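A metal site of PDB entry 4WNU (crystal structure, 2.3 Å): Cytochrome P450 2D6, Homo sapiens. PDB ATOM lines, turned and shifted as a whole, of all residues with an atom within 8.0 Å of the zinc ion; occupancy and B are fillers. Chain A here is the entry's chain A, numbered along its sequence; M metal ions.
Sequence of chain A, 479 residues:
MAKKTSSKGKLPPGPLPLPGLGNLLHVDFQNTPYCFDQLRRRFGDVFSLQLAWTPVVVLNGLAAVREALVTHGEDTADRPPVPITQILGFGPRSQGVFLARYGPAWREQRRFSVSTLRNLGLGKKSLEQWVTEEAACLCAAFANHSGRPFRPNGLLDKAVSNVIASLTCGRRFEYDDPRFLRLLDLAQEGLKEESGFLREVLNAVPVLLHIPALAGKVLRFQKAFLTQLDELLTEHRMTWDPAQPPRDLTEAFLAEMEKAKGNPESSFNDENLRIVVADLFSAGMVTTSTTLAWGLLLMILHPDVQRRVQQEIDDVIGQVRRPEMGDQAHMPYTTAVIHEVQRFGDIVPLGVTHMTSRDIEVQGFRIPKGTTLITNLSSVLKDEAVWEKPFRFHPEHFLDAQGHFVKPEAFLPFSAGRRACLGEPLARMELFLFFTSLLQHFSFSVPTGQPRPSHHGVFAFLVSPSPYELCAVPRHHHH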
ATOM      1  N   ALA A 165       7.359 -24.678   2.471  1.00  0.00           N
ATOM      2  CA  ALA A 165       8.099 -23.464   2.789  1.00  0.00           C
ATOM      3  C   ALA A 165       9.205 -23.284   1.774  1.00  0.00           C
ATOM      4  O   ALA A 165       9.441 -22.188   1.287  1.00  0.00           O
ATOM      5  CB  ALA A 165       8.670 -23.522   4.248  1.00  0.00           C
ATOM      6  N   SER A 166       9.884 -24.386   1.445  1.00  0.00           N
ATOM      7  CA  SER A 166      10.962 -24.335   0.466  1.00  0.00           C
ATOM      8  C   SER A 166      10.468 -23.962  -0.933  1.00  0.00           C
ATOM      9  O   SER A 166      11.084 -23.141  -1.606  1.00  0.00           O
ATOM     10  CB  SER A 166      11.686 -25.680   0.405  1.00  0.00           C
ATOM     11  OG  SER A 166      12.386 -25.894   1.618  1.00  0.00           O
ATOM     12  N   LEU A 167       9.370 -24.582  -1.355  1.00  0.00           N
ATOM     13  CA  LEU A 167       8.760 -24.297  -2.657  1.00  0.00           C
ATOM     14  C   LEU A 167       8.262 -22.857  -2.758  1.00  0.00           C
ATOM     15  O   LEU A 167       8.371 -22.229  -3.817  1.00  0.00           O
ATOM     16  CB  LEU A 167       7.593 -25.262  -2.914  1.00  0.00           C
ATOM     17  CG  LEU A 167       6.492 -24.823  -3.887  1.00  0.00           C
ATOM     18  CD1 LEU A 167       6.997 -24.782  -5.343  1.00  0.00           C
ATOM     19  CD2 LEU A 167       5.252 -25.734  -3.774  1.00  0.00           C
ATOM     20  N   THR A 168       7.692 -22.349  -1.661  1.00  0.00           N
ATOM     21  CA  THR A 168       6.964 -21.095  -1.730  1.00  0.00           C
ATOM     22  C   THR A 168       7.848 -19.913  -1.378  1.00  0.00           C
ATOM     23  O   THR A 168       7.762 -18.878  -2.040  1.00  0.00           O
ATOM     24  CB  THR A 168       5.735 -21.063  -0.817  1.00  0.00           C
ATOM     25  OG1 THR A 168       6.123 -21.305   0.543  1.00  0.00           O
ATOM     26  CG2 THR A 168       4.694 -22.080  -1.282  1.00  0.00           C
ATOM     27  N   CYS A 169       8.693 -20.070  -0.354  1.00  0.00           N
ATOM     28  CA  CYS A 169       9.531 -18.983   0.118  1.00  0.00           C
ATOM     29  C   CYS A 169      11.024 -19.258  -0.033  1.00  0.00           C
ATOM     30  O   CYS A 169      11.817 -18.418   0.318  1.00  0.00           O
ATOM     31  CB  CYS A 169       9.249 -18.664   1.593  1.00  0.00           C
ATOM     32  SG  CYS A 169       7.557 -18.200   2.087  1.00  0.00           S
ATOM     33  N   GLY A 170      11.411 -20.433  -0.521  1.00  0.00           N
ATOM     34  CA  GLY A 170      12.826 -20.735  -0.641  1.00  0.00           C
ATOM     35  C   GLY A 170      13.592 -20.763   0.692  1.00  0.00           C
ATOM     36  O   GLY A 170      14.763 -20.349   0.764  1.00  0.00           O
ATOM     37  N   ARG A 171      12.938 -21.253   1.739  1.00  0.00           N
ATOM     38  CA  ARG A 171      13.607 -21.458   3.047  1.00  0.00           C
ATOM     39  C   ARG A 171      12.922 -22.568   3.813  1.00  0.00           C
ATOM     40  O   ARG A 171      11.761 -22.885   3.524  1.00  0.00           O
ATOM     41  CB  ARG A 171      13.578 -20.195   3.905  1.00  0.00           C
ATOM     42  CG  ARG A 171      12.174 -19.824   4.370  1.00  0.00           C
ATOM     43  CD  ARG A 171      12.165 -18.877   5.551  1.00  0.00           C
ATOM     44  NE  ARG A 171      12.787 -19.480   6.731  1.00  0.00           N
ATOM     45  CZ  ARG A 171      13.059 -18.824   7.844  1.00  0.00           C
ATOM     46  NH1 ARG A 171      12.796 -17.522   7.936  1.00  0.00           N
ATOM     47  NH2 ARG A 171      13.637 -19.443   8.871  1.00  0.00           N
ATOM     48  N   HIS A 236      10.106 -12.024   3.040  1.00  0.00           N
ATOM     49  CA  HIS A 236      10.644 -12.591   1.820  1.00  0.00           C
ATOM     50  C   HIS A 236      10.733 -11.534   0.729  1.00  0.00           C
ATOM     51  O   HIS A 236      11.637 -11.543  -0.079  1.00  0.00           O
ATOM     52  CB  HIS A 236       9.764 -13.750   1.355  1.00  0.00           C
ATOM     53  CG  HIS A 236      10.310 -14.498   0.182  1.00  0.00           C
ATOM     54  ND1 HIS A 236       9.528 -14.851  -0.886  1.00  0.00           N
ATOM     55  CD2 HIS A 236      11.554 -14.942  -0.095  1.00  0.00           C
ATOM     56  CE1 HIS A 236      10.263 -15.509  -1.766  1.00  0.00           C
ATOM     57  NE2 HIS A 236      11.495 -15.573  -1.322  1.00  0.00           N
ATOM     58  N   ARG A 237       9.792 -10.589   0.744  1.00  0.00           N
ATOM     59  CA  ARG A 237       9.747  -9.618  -0.325  1.00  0.00           C
ATOM     60  C   ARG A 237      10.935  -8.677  -0.181  1.00  0.00           C
ATOM     61  O   ARG A 237      11.425  -8.143  -1.174  1.00  0.00           O
ATOM     62  CB  ARG A 237       8.414  -8.864  -0.335  1.00  0.00           C
ATOM     63  CG  ARG A 237       8.383  -7.711  -1.307  1.00  0.00           C
ATOM     64  CD  ARG A 237       7.047  -7.521  -1.999  1.00  0.00           C
ATOM     65  NE  ARG A 237       5.917  -8.009  -1.216  1.00  0.00           N
ATOM     66  CZ  ARG A 237       4.660  -7.971  -1.641  1.00  0.00           C
ATOM     67  NH1 ARG A 237       4.396  -7.459  -2.837  1.00  0.00           N
ATOM     68  NH2 ARG A 237       3.663  -8.452  -0.891  1.00  0.00           N
ATOM     69  N   THR A 239      13.976  -9.750   0.837  1.00  0.00           N
ATOM     70  CA  THR A 239      15.203 -10.440   0.455  1.00  0.00           C
ATOM     71  C   THR A 239      15.246 -10.923  -1.006  1.00  0.00           C
ATOM     72  O   THR A 239      16.296 -11.346  -1.465  1.00  0.00           O
ATOM     73  CB  THR A 239      15.455 -11.668   1.347  1.00  0.00           C
ATOM     74  OG1 THR A 239      14.367 -12.575   1.218  1.00  0.00           O
ATOM     75  CG2 THR A 239      15.624 -11.239   2.796  1.00  0.00           C
ATOM     76  N   TRP A 240      14.105 -10.905  -1.696  1.00  0.00           N
ATOM     77  CA  TRP A 240      14.035 -11.170  -3.144  1.00  0.00           C
ATOM     78  C   TRP A 240      15.119 -10.437  -3.937  1.00  0.00           C
ATOM     79  O   TRP A 240      15.269  -9.215  -3.792  1.00  0.00           O
ATOM     80  CB  TRP A 240      12.672 -10.751  -3.688  1.00  0.00           C
ATOM     81  CG  TRP A 240      12.440 -10.980  -5.157  1.00  0.00           C
ATOM     82  CD1 TRP A 240      13.030 -11.931  -5.941  1.00  0.00           C
ATOM     83  CD2 TRP A 240      11.543 -10.262  -6.012  1.00  0.00           C
ATOM     84  NE1 TRP A 240      12.553 -11.843  -7.234  1.00  0.00           N
ATOM     85  CE2 TRP A 240      11.638 -10.823  -7.299  1.00  0.00           C
ATOM     86  CE3 TRP A 240      10.686  -9.176  -5.814  1.00  0.00           C
ATOM     87  CZ2 TRP A 240      10.906 -10.351  -8.386  1.00  0.00           C
ATOM     88  CZ3 TRP A 240       9.949  -8.705  -6.885  1.00  0.00           C
ATOM     89  CH2 TRP A 240      10.065  -9.300  -8.163  1.00  0.00           C
ATOM     90  N   ASP A 241      15.877 -11.167  -4.758  1.00  0.00           N
ATOM     91  CA  ASP A 241      16.785 -10.546  -5.730  1.00  0.00           C
ATOM     92  C   ASP A 241      16.195 -10.638  -7.135  1.00  0.00           C
ATOM     93  O   ASP A 241      16.372 -11.642  -7.822  1.00  0.00           O
ATOM     94  CB  ASP A 241      18.158 -11.212  -5.689  1.00  0.00           C
ATOM     95  CG  ASP A 241      19.209 -10.415  -6.436  1.00  0.00           C
ATOM     96  OD1 ASP A 241      20.396 -10.804  -6.430  1.00  0.00           O
ATOM     97  OD2 ASP A 241      18.829  -9.407  -7.037  1.00  0.00           O
ATOM     98  N   PRO A 245      17.261 -15.147 -11.639  1.00  0.00           N
ATOM     99  CA  PRO A 245      16.096 -16.006 -11.875  1.00  0.00           C
ATOM    100  C   PRO A 245      15.400 -16.329 -10.557  1.00  0.00           C
ATOM    101  O   PRO A 245      16.073 -16.389  -9.537  1.00  0.00           O
ATOM    102  CB  PRO A 245      16.719 -17.265 -12.502  1.00  0.00           C
ATOM    103  CG  PRO A 245      17.921 -16.713 -13.239  1.00  0.00           C
ATOM    104  CD  PRO A 245      18.472 -15.674 -12.295  1.00  0.00           C
ATOM    105  N   PRO A 246      14.067 -16.469 -10.582  1.00  0.00           N
ATOM    106  CA  PRO A 246      13.336 -16.756  -9.339  1.00  0.00           C
ATOM    107  C   PRO A 246      13.812 -18.029  -8.653  1.00  0.00           C
ATOM    108  O   PRO A 246      13.964 -19.060  -9.321  1.00  0.00           O
ATOM    109  CB  PRO A 246      11.893 -16.883  -9.826  1.00  0.00           C
ATOM    110  CG  PRO A 246      11.828 -16.009 -11.061  1.00  0.00           C
ATOM    111  CD  PRO A 246      13.171 -16.153 -11.708  1.00  0.00           C
ATOM    112  N   ARG A 247      14.033 -17.962  -7.342  1.00  0.00           N
ATOM    113  CA  ARG A 247      14.497 -19.116  -6.564  1.00  0.00           C
ATOM    114  C   ARG A 247      13.357 -20.012  -6.083  1.00  0.00           C
ATOM    115  O   ARG A 247      13.566 -21.120  -5.628  1.00  0.00           O
ATOM    116  CB  ARG A 247      15.274 -18.648  -5.324  1.00  0.00           C
ATOM    117  CG  ARG A 247      16.689 -18.177  -5.537  1.00  0.00           C
ATOM    118  CD  ARG A 247      17.536 -18.563  -4.325  1.00  0.00           C
ATOM    119  NE  ARG A 247      16.725 -18.530  -3.107  1.00  0.00           N
ATOM    120  CZ  ARG A 247      16.501 -19.564  -2.288  1.00  0.00           C
ATOM    121  NH1 ARG A 247      17.041 -20.757  -2.529  1.00  0.00           N
ATOM    122  NH2 ARG A 247      15.728 -19.391  -1.236  1.00  0.00           N
ATOM    123  N   ASP A 248      12.133 -19.489  -6.139  1.00  0.00           N
ATOM    124  CA  ASP A 248      10.982 -20.149  -5.582  1.00  0.00           C
ATOM    125  C   ASP A 248       9.755 -19.535  -6.177  1.00  0.00           C
ATOM    126  O   ASP A 248       9.850 -18.582  -6.928  1.00  0.00           O
ATOM    127  CB  ASP A 248      10.949 -20.027  -4.058  1.00  0.00           C
ATOM    128  CG  ASP A 248      11.211 -18.621  -3.592  1.00  0.00           C
ATOM    129  OD1 ASP A 248      10.518 -17.671  -4.008  1.00  0.00           O
ATOM    130  OD2 ASP A 248      12.144 -18.447  -2.797  1.00  0.00           O
ATOM    131  N   LEU A 249       8.603 -20.060  -5.794  1.00  0.00           N
ATOM    132  CA  LEU A 249       7.327 -19.757  -6.432  1.00  0.00           C
ATOM    133  C   LEU A 249       6.826 -18.356  -6.114  1.00  0.00           C
ATOM    134  O   LEU A 249       6.265 -17.696  -6.995  1.00  0.00           O
ATOM    135  CB  LEU A 249       6.282 -20.827  -6.026  1.00  0.00           C
ATOM    136  CG  LEU A 249       4.853 -20.683  -6.577  1.00  0.00           C
ATOM    137  CD1 LEU A 249       4.185 -22.029  -6.906  1.00  0.00           C
ATOM    138  CD2 LEU A 249       3.943 -19.906  -5.625  1.00  0.00           C
ATOM    139  N   THR A 250       7.015 -17.894  -4.876  1.00  0.00           N
ATOM    140  CA  THR A 250       6.656 -16.511  -4.524  1.00  0.00           C
ATOM    141  C   THR A 250       7.435 -15.515  -5.402  1.00  0.00           C
ATOM    142  O   THR A 250       6.896 -14.504  -5.867  1.00  0.00           O
ATOM    143  CB  THR A 250       6.906 -16.242  -2.994  1.00  0.00           C
ATOM    144  OG1 THR A 250       5.947 -16.991  -2.215  1.00  0.00           O
ATOM    145  CG2 THR A 250       6.799 -14.780  -2.636  1.00  0.00           C
ATOM    146  N   GLU A 251       8.703 -15.807  -5.663  1.00  0.00           N
ATOM    147  CA  GLU A 251       9.513 -14.911  -6.475  1.00  0.00           C
ATOM    148  C   GLU A 251       9.051 -14.924  -7.923  1.00  0.00           C
ATOM    149  O   GLU A 251       9.045 -13.877  -8.593  1.00  0.00           O
ATOM    150  CB  GLU A 251      10.999 -15.271  -6.374  1.00  0.00           C
ATOM    151  CG  GLU A 251      11.607 -14.897  -4.977  1.00  0.00           C
ATOM    152  CD  GLU A 251      13.046 -15.337  -4.841  1.00  0.00           C
ATOM    153  OE1 GLU A 251      13.695 -15.550  -5.892  1.00  0.00           O
ATOM    154  OE2 GLU A 251      13.531 -15.436  -3.676  1.00  0.00           O
ATOM    155  N   ALA A 252       8.664 -16.103  -8.404  1.00  0.00           N
ATOM    156  CA  ALA A 252       8.132 -16.197  -9.764  1.00  0.00           C
ATOM    157  C   ALA A 252       6.846 -15.364  -9.871  1.00  0.00           C
ATOM    158  O   ALA A 252       6.639 -14.653 -10.843  1.00  0.00           O
ATOM    159  CB  ALA A 252       7.884 -17.665 -10.153  1.00  0.00           C
ATOM    160  N   LEU A 254       5.948 -12.772  -7.896  1.00  0.00           N
ATOM    161  CA  LEU A 254       6.269 -11.358  -7.704  1.00  0.00           C
ATOM    162  C   LEU A 254       6.713 -10.775  -9.046  1.00  0.00           C
ATOM    163  O   LEU A 254       6.248  -9.716  -9.442  1.00  0.00           O
ATOM    164  CB  LEU A 254       7.341 -11.151  -6.617  1.00  0.00           C
ATOM    165  CG  LEU A 254       6.853 -11.268  -5.170  1.00  0.00           C
ATOM    166  CD1 LEU A 254       8.019 -11.431  -4.213  1.00  0.00           C
ATOM    167  CD2 LEU A 254       5.965 -10.103  -4.745  1.00  0.00           C
HETATM  168 ZN    ZN M   1      12.835 -16.457  -2.317  1.00  0.00          ZN
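Cys 169 touches the zinc ion.
Four residues have an atom within 4 Å of the zinc ion: Cys 169, His 236, Asp 248 and Glu 251.
OE2 of Glu 251 is bound to the zinc ion, 1.8 Å away.
NE2 of His 236 is bound to the zinc ion (1.9 Å).
OD2 of Asp 248 binds the zinc ion.
NE2 of His 236 sits close to O of Cys 169, 3.3 Å away.
The backbone carbonyl oxygen (O) of His 236 sits at hydrogen-bond distance from the side-chain hydroxyl (OG1) of Thr 239, 3.2 Å away.
The side-chain carboxylate of Glu 251 sits at hydrogen-bond distance from the backbone NH of Arg 247.
The side-chain carboxylate (OD2) of Asp 248 lies close to the backbone NH (N) of Gly 170.
The side-chain sulfur of Cys 169 is in hydrogen-bond range of the side-chain hydroxyl of Thr 168, at 3.8 Å.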
